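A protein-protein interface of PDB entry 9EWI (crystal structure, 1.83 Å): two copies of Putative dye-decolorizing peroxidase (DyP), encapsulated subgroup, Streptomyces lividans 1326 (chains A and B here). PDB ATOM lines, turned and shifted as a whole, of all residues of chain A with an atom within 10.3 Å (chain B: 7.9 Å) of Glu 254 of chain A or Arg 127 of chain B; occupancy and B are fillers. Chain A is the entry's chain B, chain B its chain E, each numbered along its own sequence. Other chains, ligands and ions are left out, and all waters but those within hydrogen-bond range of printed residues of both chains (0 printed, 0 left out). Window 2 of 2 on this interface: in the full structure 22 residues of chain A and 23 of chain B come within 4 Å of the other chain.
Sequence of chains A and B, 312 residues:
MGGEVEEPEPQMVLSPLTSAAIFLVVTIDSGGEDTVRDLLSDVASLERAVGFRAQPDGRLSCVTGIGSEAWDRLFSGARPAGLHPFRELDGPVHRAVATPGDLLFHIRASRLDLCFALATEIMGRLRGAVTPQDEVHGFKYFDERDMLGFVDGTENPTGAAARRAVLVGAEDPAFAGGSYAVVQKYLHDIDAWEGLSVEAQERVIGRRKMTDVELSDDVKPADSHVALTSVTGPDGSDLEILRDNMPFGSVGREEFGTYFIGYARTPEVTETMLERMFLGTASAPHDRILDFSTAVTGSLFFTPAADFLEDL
Among the printed residues, merely in contact across the chains: Val 251 of chain A with Met 123 of chain B, Val 251 of chain A with Thr 120 of chain B, Val 251 of chain A with Phe 116 of chain B, Phe 256 of chain A with Thr 120 of chain B, Gly 249 of chain A with Phe 116 of chain B, Gly 252 of chain A with Pro 132 of chain B, Val 251 of chain A with Ala 119 of chain B, Phe 256 of chain A with Phe 116 of chain B, Ser 250 of chain A with Phe 116 of chain B and Met 147 of chain A with Phe 116 of chain B.
No position is printed for both chains.
The side-chain hydroxyl (OG1) of Thr 120 of chain B sits at hydrogen-bond distance from the backbone carbonyl oxygen (O) of Phe 116 of chain B (2.9 Å).
N of Ser 250 of chain A lies within hydrogen-bond range of O of Glu 255 of chain A (2.9 Å).
OG of Ser 250 of chain A lies within hydrogen-bond range of N of Arg 253 of chain A, at 3.3 Å.
The backbone carbonyl oxygen of Phe 256 of chain A sits at hydrogen-bond distance from the backbone NH of His 188 of chain A, 2.9 Å away.
Of the 19 printed residues of chain A, 7 touch a printed residue of chain B.
Hydrophobic or aromatic side chains of chain A that line the printed part of chain B: Met 147, Val 251 and Phe 256.
Among the printed residues, 15 pairs touch across the chains.
Among the printed residues, Asp or Glu carboxylates within 4 Å of a Lys or Arg side-chain nitrogen of the other chain: Glu 254 of chain A with Arg 127 of chain B (3.6 Å).
Of the printed residues of chain B, Met 147 of chain A touches Phe 116 (3.9 Å).
Asp 191 of chain A touches none of the printed residues of chain B.
Of the printed residues of chain B, Gly 249 of chain A touches Phe 116 (3.7 Å).
Printed residues of chain B within 4 Å of Ser 250 of chain A: Phe 116 and Glu 135.
Glu 254 of chain A touches just one residue of chain B: Arg 127 (3.2 Å).
Thr 35 of chain B touches none of the printed residues of chain A.
Printed residues of chain A within 4 Å of Phe 116 of chain B: Met 147 (3.9 Å), Gly 249 (3.7 Å), Ser 250 (3.8 Å), Val 251 (3.6 Å) and Phe 256 (3.8 Å).
No residue of chain A comes within 4 Å of Gly 124 of chain B.
No residue of chain A comes within 4 Å of Leu 126 of chain B.
Arg 127 of chain B touches just these residues of chain A: Val 251 (3.0 Å) and Glu 254 (3.2 Å).
No residue of chain A comes within 4 Å of Gly 128 of chain B.
Of the printed residues of chain A, Pro 132 of chain B touches Gly 252 (3.7 Å).
The nearest residue of chain B that does not touch Glu 254 of chain A is Glu 135 of chain B (6.2 Å).
The nearest printed residue of chain A that does not touch Pro 132 of chain B is Arg 253 of chain A (5.5 Å).
The side-chain hydroxyl (OG) of Ser 250 of chain A is in hydrogen-bond range of the side-chain carboxylate (OE1) of Glu 135 of chain B, 3.1 Å away.
The guanidinium group (NE) of Arg 127 of chain B is in salt-bridge range of the side-chain carboxylate (OE2) of Glu 254 of chain A.
NH2 of Arg 127 of chain B is in hydrogen-bond range of O of Val 251 of chain A.
The side-chain carboxylate (OE2) of Glu 135 of chain B lies within hydrogen-bond range of the backbone NH (N) of Val 251 of chain A, at 3.0 Å.
N of Gly 252 of chain A sits at hydrogen-bond distance from OE1 of Glu 135 of chain B, 2.7 Å away.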
ATOM      1  N   MET A 147       1.963  22.326 -28.221  1.00  0.00           N
ATOM      2  CA  MET A 147       3.412  22.357 -28.047  1.00  0.00           C
ATOM      3  C   MET A 147       4.134  22.364 -29.422  1.00  0.00           C
ATOM      4  O   MET A 147       5.247  22.824 -29.533  1.00  0.00           O
ATOM      5  CB  MET A 147       3.782  21.160 -27.143  1.00  0.00           C
ATOM      6  CG  MET A 147       5.190  21.223 -26.558  1.00  0.00           C
ATOM      7  SD  MET A 147       5.422  22.664 -25.497  1.00  0.00           S
ATOM      8  CE  MET A 147       4.827  22.209 -23.858  1.00  0.00           C
ATOM      9  N   TYR A 186       1.993  12.170 -24.155  1.00  0.00           N
ATOM     10  CA  TYR A 186       2.992  12.157 -25.210  1.00  0.00           C
ATOM     11  C   TYR A 186       4.121  13.102 -24.820  1.00  0.00           C
ATOM     12  O   TYR A 186       3.860  14.224 -24.377  1.00  0.00           O
ATOM     13  CB  TYR A 186       2.416  12.618 -26.551  1.00  0.00           C
ATOM     14  CG  TYR A 186       1.573  11.586 -27.277  1.00  0.00           C
ATOM     15  CD1 TYR A 186       2.157  10.674 -28.139  1.00  0.00           C
ATOM     16  CD2 TYR A 186       0.192  11.537 -27.120  1.00  0.00           C
ATOM     17  CE1 TYR A 186       1.392   9.735 -28.801  1.00  0.00           C
ATOM     18  CE2 TYR A 186      -0.585  10.614 -27.805  1.00  0.00           C
ATOM     19  CZ  TYR A 186       0.024   9.699 -28.636  1.00  0.00           C
ATOM     20  OH  TYR A 186      -0.737   8.780 -29.292  1.00  0.00           O
ATOM     21  N   LEU A 187       5.356  12.650 -25.072  1.00  0.00           N
ATOM     22  CA  LEU A 187       6.501  13.544 -25.027  1.00  0.00           C
ATOM     23  C   LEU A 187       6.980  13.810 -26.452  1.00  0.00           C
ATOM     24  O   LEU A 187       7.016  12.885 -27.255  1.00  0.00           O
ATOM     25  CB  LEU A 187       7.570  12.896 -24.153  1.00  0.00           C
ATOM     26  CG  LEU A 187       7.252  12.789 -22.656  1.00  0.00           C
ATOM     27  CD1 LEU A 187       8.429  12.082 -21.986  1.00  0.00           C
ATOM     28  CD2 LEU A 187       7.068  14.145 -21.975  1.00  0.00           C
ATOM     29  N   HIS A 188       7.424  15.049 -26.725  1.00  0.00           N
ATOM     30  CA  HIS A 188       7.820  15.417 -28.061  1.00  0.00           C
ATOM     31  C   HIS A 188       9.329  15.577 -28.140  1.00  0.00           C
ATOM     32  O   HIS A 188       9.949  15.927 -27.169  1.00  0.00           O
ATOM     33  CB  HIS A 188       7.180  16.735 -28.485  1.00  0.00           C
ATOM     34  CG  HIS A 188       5.729  16.654 -28.602  1.00  0.00           C
ATOM     35  ND1 HIS A 188       5.122  15.898 -29.566  1.00  0.00           N
ATOM     36  CD2 HIS A 188       4.762  17.212 -27.868  1.00  0.00           C
ATOM     37  CE1 HIS A 188       3.800  16.013 -29.414  1.00  0.00           C
ATOM     38  NE2 HIS A 188       3.562  16.804 -28.382  1.00  0.00           N
ATOM     39  N   ASP A 189       9.875  15.290 -29.314  1.00  0.00           N
ATOM     40  CA  ASP A 189      11.236  15.645 -29.660  1.00  0.00           C
ATOM     41  C   ASP A 189      11.202  17.011 -30.351  1.00  0.00           C
ATOM     42  O   ASP A 189      11.116  17.107 -31.575  1.00  0.00           O
ATOM     43  CB  ASP A 189      11.862  14.535 -30.492  1.00  0.00           C
ATOM     44  CG  ASP A 189      13.316  14.772 -30.830  1.00  0.00           C
ATOM     45  OD1 ASP A 189      13.826  15.871 -30.579  1.00  0.00           O
ATOM     46  OD2 ASP A 189      13.906  13.852 -31.371  1.00  0.00           O
ATOM     47  N   ILE A 190      11.290  18.061 -29.544  1.00  0.00           N
ATOM     48  CA  ILE A 190      11.160  19.417 -30.041  1.00  0.00           C
ATOM     49  C   ILE A 190      12.318  19.804 -30.949  1.00  0.00           C
ATOM     50  O   ILE A 190      12.093  20.532 -31.913  1.00  0.00           O
ATOM     51  CB  ILE A 190      10.958  20.426 -28.887  1.00  0.00           C
ATOM     52  CG1 ILE A 190       9.571  20.231 -28.289  1.00  0.00           C
ATOM     53  CG2 ILE A 190      11.107  21.871 -29.385  1.00  0.00           C
ATOM     54  CD1 ILE A 190       8.400  20.503 -29.274  1.00  0.00           C
ATOM     55  N   ASP A 191      13.535  19.352 -30.649  1.00  0.00           N
ATOM     56  CA  ASP A 191      14.671  19.711 -31.494  1.00  0.00           C
ATOM     57  C   ASP A 191      14.487  19.159 -32.902  1.00  0.00           C
ATOM     58  O   ASP A 191      14.765  19.838 -33.869  1.00  0.00           O
ATOM     59  CB  ASP A 191      15.984  19.170 -30.961  1.00  0.00           C
ATOM     60  CG  ASP A 191      16.522  19.888 -29.741  1.00  0.00           C
ATOM     61  OD1 ASP A 191      15.971  20.943 -29.370  1.00  0.00           O
ATOM     62  OD2 ASP A 191      17.510  19.388 -29.207  1.00  0.00           O
ATOM     63  N   ALA A 192      14.025  17.914 -33.027  1.00  0.00           N
ATOM     64  CA  ALA A 192      13.788  17.369 -34.346  1.00  0.00           C
ATOM     65  C   ALA A 192      12.680  18.167 -35.054  1.00  0.00           C
ATOM     66  O   ALA A 192      12.821  18.493 -36.224  1.00  0.00           O
ATOM     67  CB  ALA A 192      13.433  15.902 -34.226  1.00  0.00           C
ATOM     68  N   GLU A 194      11.649  21.231 -34.691  1.00  0.00           N
ATOM     69  CA  GLU A 194      12.024  22.595 -35.036  1.00  0.00           C
ATOM     70  C   GLU A 194      13.034  22.607 -36.173  1.00  0.00           C
ATOM     71  O   GLU A 194      13.203  23.612 -36.835  1.00  0.00           O
ATOM     72  CB  GLU A 194      12.395  23.414 -33.806  1.00  0.00           C
ATOM     73  CG  GLU A 194      11.120  24.040 -33.237  1.00  0.00           C
ATOM     74  CD  GLU A 194      11.281  24.666 -31.874  1.00  0.00           C
ATOM     75  OE1 GLU A 194      12.415  24.820 -31.358  1.00  0.00           O
ATOM     76  OE2 GLU A 194      10.230  24.985 -31.314  1.00  0.00           O
ATOM     77  N   PHE A 248       2.039  20.471 -21.640  1.00  0.00           N
ATOM     78  CA  PHE A 248       2.606  20.479 -20.304  1.00  0.00           C
ATOM     79  C   PHE A 248       4.108  20.397 -20.473  1.00  0.00           C
ATOM     80  O   PHE A 248       4.592  20.034 -21.546  1.00  0.00           O
ATOM     81  CB  PHE A 248       2.093  19.327 -19.453  1.00  0.00           C
ATOM     82  CG  PHE A 248       2.586  17.969 -19.914  1.00  0.00           C
ATOM     83  CD1 PHE A 248       1.917  17.265 -20.907  1.00  0.00           C
ATOM     84  CD2 PHE A 248       3.729  17.403 -19.363  1.00  0.00           C
ATOM     85  CE1 PHE A 248       2.399  16.036 -21.351  1.00  0.00           C
ATOM     86  CE2 PHE A 248       4.210  16.180 -19.813  1.00  0.00           C
ATOM     87  CZ  PHE A 248       3.543  15.507 -20.802  1.00  0.00           C
ATOM     88  N   GLY A 249       4.830  20.704 -19.399  1.00  0.00           N
ATOM     89  CA  GLY A 249       6.234  20.390 -19.428  1.00  0.00           C
ATOM     90  C   GLY A 249       7.043  20.973 -18.292  1.00  0.00           C
ATOM     91  O   GLY A 249       6.555  21.606 -17.368  1.00  0.00           O
ATOM     92  N   SER A 250       8.350  20.802 -18.475  1.00  0.00           N
ATOM     93  CA  SER A 250       9.350  21.291 -17.543  1.00  0.00           C
ATOM     94  C   SER A 250      10.580  21.674 -18.360  1.00  0.00           C
ATOM     95  O   SER A 250      11.136  20.868 -19.091  1.00  0.00           O
ATOM     96  CB  SER A 250       9.608  20.213 -16.518  1.00  0.00           C
ATOM     97  OG  SER A 250      10.920  20.337 -16.015  1.00  0.00           O
ATOM     98  N   VAL A 251      10.973  22.936 -18.322  1.00  0.00           N
ATOM     99  CA  VAL A 251      12.091  23.425 -19.130  1.00  0.00           C
ATOM    100  C   VAL A 251      13.415  22.818 -18.621  1.00  0.00           C
ATOM    101  O   VAL A 251      14.306  22.499 -19.387  1.00  0.00           O
ATOM    102  CB  VAL A 251      11.912  24.944 -18.921  1.00  0.00           C
ATOM    103  CG1 VAL A 251      13.162  25.757 -18.887  1.00  0.00           C
ATOM    104  CG2 VAL A 251      10.900  25.541 -19.879  1.00  0.00           C
ATOM    105  N   GLY A 252      13.524  22.618 -17.295  1.00  0.00           N
ATOM    106  CA  GLY A 252      14.736  22.148 -16.663  1.00  0.00           C
ATOM    107  C   GLY A 252      15.051  20.721 -17.055  1.00  0.00           C
ATOM    108  O   GLY A 252      16.196  20.385 -17.341  1.00  0.00           O
ATOM    109  N   ARG A 253      14.026  19.891 -17.097  1.00  0.00           N
ATOM    110  CA  ARG A 253      14.188  18.491 -17.489  1.00  0.00           C
ATOM    111  C   ARG A 253      14.008  18.290 -18.995  1.00  0.00           C
ATOM    112  O   ARG A 253      14.027  17.178 -19.470  1.00  0.00           O
ATOM    113  CB  ARG A 253      13.171  17.626 -16.752  1.00  0.00           C
ATOM    114  CG  ARG A 253      13.429  17.516 -15.261  1.00  0.00           C
ATOM    115  CD  ARG A 253      12.873  16.203 -14.698  1.00  0.00           C
ATOM    116  NE  ARG A 253      11.450  16.078 -15.028  1.00  0.00           N
ATOM    117  CZ  ARG A 253      10.475  16.919 -14.660  1.00  0.00           C
ATOM    118  NH1 ARG A 253      10.676  17.861 -13.741  1.00  0.00           N
ATOM    119  NH2 ARG A 253       9.274  16.792 -15.201  1.00  0.00           N
ATOM    120  N   GLU A 254      13.852  19.356 -19.775  1.00  0.00           N
ATOM    121  CA  GLU A 254      13.616  19.239 -21.204  1.00  0.00           C
ATOM    122  C   GLU A 254      12.435  18.328 -21.546  1.00  0.00           C
ATOM    123  O   GLU A 254      12.533  17.577 -22.493  1.00  0.00           O
ATOM    124  CB  GLU A 254      14.846  18.692 -21.905  1.00  0.00           C
ATOM    125  CG  GLU A 254      15.917  19.768 -22.036  1.00  0.00           C
ATOM    126  CD  GLU A 254      17.230  19.279 -22.607  1.00  0.00           C
ATOM    127  OE1 GLU A 254      17.132  18.838 -23.779  1.00  0.00           O
ATOM    128  OE2 GLU A 254      18.264  19.287 -21.875  1.00  0.00           O
ATOM    129  N   GLU A 255      11.335  18.395 -20.780  1.00  0.00           N
ATOM    130  CA  GLU A 255      10.107  17.715 -21.127  1.00  0.00           C
ATOM    131  C   GLU A 255       9.123  18.690 -21.768  1.00  0.00           C
ATOM    132  O   GLU A 255       8.720  19.691 -21.168  1.00  0.00           O
ATOM    133  CB  GLU A 255       9.398  17.129 -19.925  1.00  0.00           C
ATOM    134  CG  GLU A 255      10.083  15.872 -19.408  1.00  0.00           C
ATOM    135  CD  GLU A 255       9.307  15.311 -18.226  1.00  0.00           C
ATOM    136  OE1 GLU A 255       8.125  15.742 -17.951  1.00  0.00           O
ATOM    137  OE2 GLU A 255       9.969  14.488 -17.545  1.00  0.00           O
ATOM    138  N   PHE A 256       8.750  18.387 -22.999  1.00  0.00           N
ATOM    139  CA  PHE A 256       7.739  19.153 -23.694  1.00  0.00           C
ATOM    140  C   PHE A 256       6.709  18.153 -24.199  1.00  0.00           C
ATOM    141  O   PHE A 256       7.068  17.226 -24.907  1.00  0.00           O
ATOM    142  CB  PHE A 256       8.352  19.937 -24.844  1.00  0.00           C
ATOM    143  CG  PHE A 256       9.492  20.820 -24.383  1.00  0.00           C
ATOM    144  CD1 PHE A 256       9.223  22.046 -23.814  1.00  0.00           C
ATOM    145  CD2 PHE A 256      10.820  20.397 -24.499  1.00  0.00           C
ATOM    146  CE1 PHE A 256      10.265  22.853 -23.401  1.00  0.00           C
ATOM    147  CE2 PHE A 256      11.851  21.187 -24.037  1.00  0.00           C
ATOM    148  CZ  PHE A 256      11.577  22.441 -23.562  1.00  0.00           C
ATOM    149  N   GLY A 257       5.466  18.290 -23.755  1.00  0.00           N
ATOM    150  CA  GLY A 257       4.518  17.207 -23.928  1.00  0.00           C
ATOM    151  C   GLY A 257       3.138  17.710 -24.376  1.00  0.00           C
ATOM    152  O   GLY A 257       2.821  18.891 -24.314  1.00  0.00           O
ATOM    153  N   ASP B  29      28.009  26.219 -15.693  1.00  0.00           N
ATOM    154  CA  ASP B  29      29.016  25.162 -15.785  1.00  0.00           C
ATOM    155  C   ASP B  29      30.358  25.743 -16.223  1.00  0.00           C
ATOM    156  O   ASP B  29      30.434  26.880 -16.728  1.00  0.00           O
ATOM    157  CB  ASP B  29      28.619  24.088 -16.793  1.00  0.00           C
ATOM    158  CG  ASP B  29      27.340  23.338 -16.537  1.00  0.00           C
ATOM    159  OD1 ASP B  29      26.742  23.529 -15.448  1.00  0.00           O
ATOM    160  OD2 ASP B  29      26.993  22.577 -17.426  1.00  0.00           O
ATOM    161  N   THR B  35      28.422  31.873 -23.330  1.00  0.00           N
ATOM    162  CA  THR B  35      27.038  31.621 -23.686  1.00  0.00           C
ATOM    163  C   THR B  35      26.096  32.456 -22.809  1.00  0.00           C
ATOM    164  O   THR B  35      25.130  33.035 -23.297  1.00  0.00           O
ATOM    165  CB  THR B  35      26.748  30.146 -23.526  1.00  0.00           C
ATOM    166  OG1 THR B  35      27.547  29.525 -24.497  1.00  0.00           O
ATOM    167  CG2 THR B  35      25.353  29.775 -23.938  1.00  0.00           C
ATOM    168  N   PHE B 116       6.038  29.998 -19.657  1.00  0.00           N
ATOM    169  CA  PHE B 116       6.686  28.799 -20.145  1.00  0.00           C
ATOM    170  C   PHE B 116       7.344  29.053 -21.488  1.00  0.00           C
ATOM    171  O   PHE B 116       8.428  28.575 -21.753  1.00  0.00           O
ATOM    172  CB  PHE B 116       5.683  27.644 -20.141  1.00  0.00           C
ATOM    173  CG  PHE B 116       6.329  26.296 -20.380  1.00  0.00           C
ATOM    174  CD1 PHE B 116       6.828  25.556 -19.324  1.00  0.00           C
ATOM    175  CD2 PHE B 116       6.538  25.811 -21.672  1.00  0.00           C
ATOM    176  CE1 PHE B 116       7.509  24.382 -19.541  1.00  0.00           C
ATOM    177  CE2 PHE B 116       7.164  24.603 -21.882  1.00  0.00           C
ATOM    178  CZ  PHE B 116       7.642  23.883 -20.826  1.00  0.00           C
ATOM    179  N   ALA B 119      10.552  30.977 -20.730  1.00  0.00           N
ATOM    180  CA  ALA B 119      11.502  30.069 -20.102  1.00  0.00           C
ATOM    181  C   ALA B 119      12.117  29.118 -21.128  1.00  0.00           C
ATOM    182  O   ALA B 119      13.298  28.810 -21.056  1.00  0.00           O
ATOM    183  CB  ALA B 119      10.831  29.316 -18.971  1.00  0.00           C
ATOM    184  N   THR B 120      11.310  28.626 -22.087  1.00  0.00           N
ATOM    185  CA  THR B 120      11.768  27.720 -23.126  1.00  0.00           C
ATOM    186  C   THR B 120      12.836  28.399 -23.965  1.00  0.00           C
ATOM    187  O   THR B 120      13.857  27.783 -24.235  1.00  0.00           O
ATOM    188  CB  THR B 120      10.584  27.284 -24.002  1.00  0.00           C
ATOM    189  OG1 THR B 120       9.829  26.459 -23.128  1.00  0.00           O
ATOM    190  CG2 THR B 120      10.980  26.406 -25.166  1.00  0.00           C
ATOM    191  N   GLU B 121      12.587  29.647 -24.364  1.00  0.00           N
ATOM    192  CA  GLU B 121      13.539  30.339 -25.208  1.00  0.00           C
ATOM    193  C   GLU B 121      14.839  30.578 -24.422  1.00  0.00           C
ATOM    194  O   GLU B 121      15.921  30.472 -24.986  1.00  0.00           O
ATOM    195  CB  GLU B 121      13.035  31.708 -25.700  1.00  0.00           C
ATOM    196  CG  GLU B 121      11.891  31.577 -26.702  1.00  0.00           C
ATOM    197  CD  GLU B 121      12.296  31.164 -28.089  1.00  0.00           C
ATOM    198  OE1 GLU B 121      13.452  31.347 -28.437  1.00  0.00           O
ATOM    199  OE2 GLU B 121      11.461  30.674 -28.827  1.00  0.00           O
ATOM    200  N   ILE B 122      14.753  30.986 -23.145  1.00  0.00           N
ATOM    201  CA  ILE B 122      15.947  31.278 -22.372  1.00  0.00           C
ATOM    202  C   ILE B 122      16.760  29.993 -22.218  1.00  0.00           C
ATOM    203  O   ILE B 122      17.957  29.980 -22.500  1.00  0.00           O
ATOM    204  CB  ILE B 122      15.577  31.934 -21.043  1.00  0.00           C
ATOM    205  CG1 ILE B 122      15.074  33.360 -21.272  1.00  0.00           C
ATOM    206  CG2 ILE B 122      16.764  31.925 -20.077  1.00  0.00           C
ATOM    207  CD1 ILE B 122      14.397  33.977 -20.071  1.00  0.00           C
ATOM    208  N   MET B 123      16.128  28.894 -21.811  1.00  0.00           N
ATOM    209  CA  MET B 123      16.886  27.690 -21.529  1.00  0.00           C
ATOM    210  C   MET B 123      17.422  27.073 -22.810  1.00  0.00           C
ATOM    211  O   MET B 123      18.441  26.391 -22.778  1.00  0.00           O
ATOM    212  CB  MET B 123      16.069  26.659 -20.771  1.00  0.00           C
ATOM    213  CG  MET B 123      15.941  27.071 -19.309  1.00  0.00           C
ATOM    214  SD  MET B 123      17.480  26.946 -18.352  1.00  0.00           S
ATOM    215  CE  MET B 123      18.090  25.349 -18.914  1.00  0.00           C
ATOM    216  N   GLY B 124      16.746  27.342 -23.935  1.00  0.00           N
ATOM    217  CA  GLY B 124      17.208  26.886 -25.241  1.00  0.00           C
ATOM    218  C   GLY B 124      18.549  27.494 -25.593  1.00  0.00           C
ATOM    219  O   GLY B 124      19.398  26.799 -26.117  1.00  0.00           O
ATOM    220  N   ARG B 125      18.740  28.764 -25.244  1.00  0.00           N
ATOM    221  CA  ARG B 125      19.986  29.458 -25.517  1.00  0.00           C
ATOM    222  C   ARG B 125      21.069  29.050 -24.511  1.00  0.00           C
ATOM    223  O   ARG B 125      22.220  29.241 -24.779  1.00  0.00           O
ATOM    224  CB  ARG B 125      19.784  30.968 -25.410  1.00  0.00           C
ATOM    225  CG  ARG B 125      18.734  31.547 -26.350  1.00  0.00           C
ATOM    226  CD  ARG B 125      19.146  31.959 -27.760  1.00  0.00           C
ATOM    227  NE  ARG B 125      20.398  32.721 -27.688  1.00  0.00           N
ATOM    228  CZ  ARG B 125      20.468  34.064 -27.673  1.00  0.00           C
ATOM    229  NH1 ARG B 125      19.481  34.796 -28.182  1.00  0.00           N
ATOM    230  NH2 ARG B 125      21.543  34.640 -27.149  1.00  0.00           N
ATOM    231  N   LEU B 126      20.711  28.487 -23.366  1.00  0.00           N
ATOM    232  CA  LEU B 126      21.677  28.187 -22.328  1.00  0.00           C
ATOM    233  C   LEU B 126      22.039  26.719 -22.317  1.00  0.00           C
ATOM    234  O   LEU B 126      22.853  26.360 -21.493  1.00  0.00           O
ATOM    235  CB  LEU B 126      21.132  28.624 -20.959  1.00  0.00           C
ATOM    236  CG  LEU B 126      21.014  30.143 -20.741  1.00  0.00           C
ATOM    237  CD1 LEU B 126      20.464  30.465 -19.382  1.00  0.00           C
ATOM    238  CD2 LEU B 126      22.322  30.879 -20.904  1.00  0.00           C
ATOM    239  N   ARG B 127      21.367  25.873 -23.108  1.00  0.00           N
ATOM    240  CA  ARG B 127      21.566  24.426 -23.058  1.00  0.00           C
ATOM    241  C   ARG B 127      23.070  24.142 -23.135  1.00  0.00           C
ATOM    242  O   ARG B 127      23.797  24.695 -23.965  1.00  0.00           O
ATOM    243  CB  ARG B 127      20.994  23.657 -24.256  1.00  0.00           C
ATOM    244  CG  ARG B 127      19.516  23.318 -24.396  1.00  0.00           C
ATOM    245  CD  ARG B 127      18.923  22.436 -23.295  1.00  0.00           C
ATOM    246  NE  ARG B 127      17.453  22.543 -23.176  1.00  0.00           N
ATOM    247  CZ  ARG B 127      16.736  22.849 -22.060  1.00  0.00           C
ATOM    248  NH1 ARG B 127      17.298  22.920 -20.865  1.00  0.00           N
ATOM    249  NH2 ARG B 127      15.436  23.085 -22.128  1.00  0.00           N
ATOM    250  N   GLY B 128      23.590  23.310 -22.236  1.00  0.00           N
ATOM    251  CA  GLY B 128      25.001  22.938 -22.317  1.00  0.00           C
ATOM    252  C   GLY B 128      25.911  23.938 -21.625  1.00  0.00           C
ATOM    253  O   GLY B 128      27.068  23.651 -21.448  1.00  0.00           O
ATOM    254  N   ALA B 129      25.421  25.101 -21.189  1.00  0.00           N
ATOM    255  CA  ALA B 129      26.237  26.022 -20.404  1.00  0.00           C
ATOM    256  C   ALA B 129      25.855  26.059 -18.928  1.00  0.00           C
ATOM    257  O   ALA B 129      26.634  26.606 -18.169  1.00  0.00           O
ATOM    258  CB  ALA B 129      26.175  27.410 -20.982  1.00  0.00           C
ATOM    259  N   VAL B 130      24.655  25.587 -18.556  1.00  0.00           N
ATOM    260  CA  VAL B 130      24.146  25.749 -17.198  1.00  0.00           C
ATOM    261  C   VAL B 130      23.572  24.432 -16.688  1.00  0.00           C
ATOM    262  O   VAL B 130      23.266  23.549 -17.461  1.00  0.00           O
ATOM    263  CB  VAL B 130      23.098  26.864 -17.093  1.00  0.00           C
ATOM    264  CG1 VAL B 130      23.591  28.197 -17.650  1.00  0.00           C
ATOM    265  CG2 VAL B 130      21.800  26.474 -17.780  1.00  0.00           C
ATOM    266  N   THR B 131      23.401  24.315 -15.373  1.00  0.00           N
ATOM    267  CA  THR B 131      22.781  23.150 -14.752  1.00  0.00           C
ATOM    268  C   THR B 131      21.593  23.655 -13.966  1.00  0.00           C
ATOM    269  O   THR B 131      21.749  24.558 -13.147  1.00  0.00           O
ATOM    270  CB  THR B 131      23.775  22.392 -13.863  1.00  0.00           C
ATOM    271  OG1 THR B 131      24.769  21.842 -14.744  1.00  0.00           O
ATOM    272  CG2 THR B 131      23.107  21.298 -13.055  1.00  0.00           C
ATOM    273  N   PRO B 132      20.368  23.130 -14.196  1.00  0.00           N
ATOM    274  CA  PRO B 132      19.196  23.602 -13.437  1.00  0.00           C
ATOM    275  C   PRO B 132      19.330  23.244 -11.975  1.00  0.00           C
ATOM    276  O   PRO B 132      19.679  22.131 -11.687  1.00  0.00           O
ATOM    277  CB  PRO B 132      18.005  22.847 -14.062  1.00  0.00           C
ATOM    278  CG  PRO B 132      18.570  22.393 -15.383  1.00  0.00           C
ATOM    279  CD  PRO B 132      20.033  22.060 -15.151  1.00  0.00           C
ATOM    280  N   GLU B 135      13.258  24.745 -10.426  1.00  0.00           N
ATOM    281  CA  GLU B 135      12.230  25.176 -11.363  1.00  0.00           C
ATOM    282  C   GLU B 135      10.885  25.087 -10.652  1.00  0.00           C
ATOM    283  O   GLU B 135      10.512  24.043 -10.208  1.00  0.00           O
ATOM    284  CB  GLU B 135      12.208  24.314 -12.624  1.00  0.00           C
ATOM    285  CG  GLU B 135      11.097  24.708 -13.601  1.00  0.00           C
ATOM    286  CD  GLU B 135      11.096  23.910 -14.900  1.00  0.00           C
ATOM    287  OE1 GLU B 135      12.000  23.033 -15.083  1.00  0.00           O
ATOM    288  OE2 GLU B 135      10.207  24.200 -15.752  1.00  0.00           O
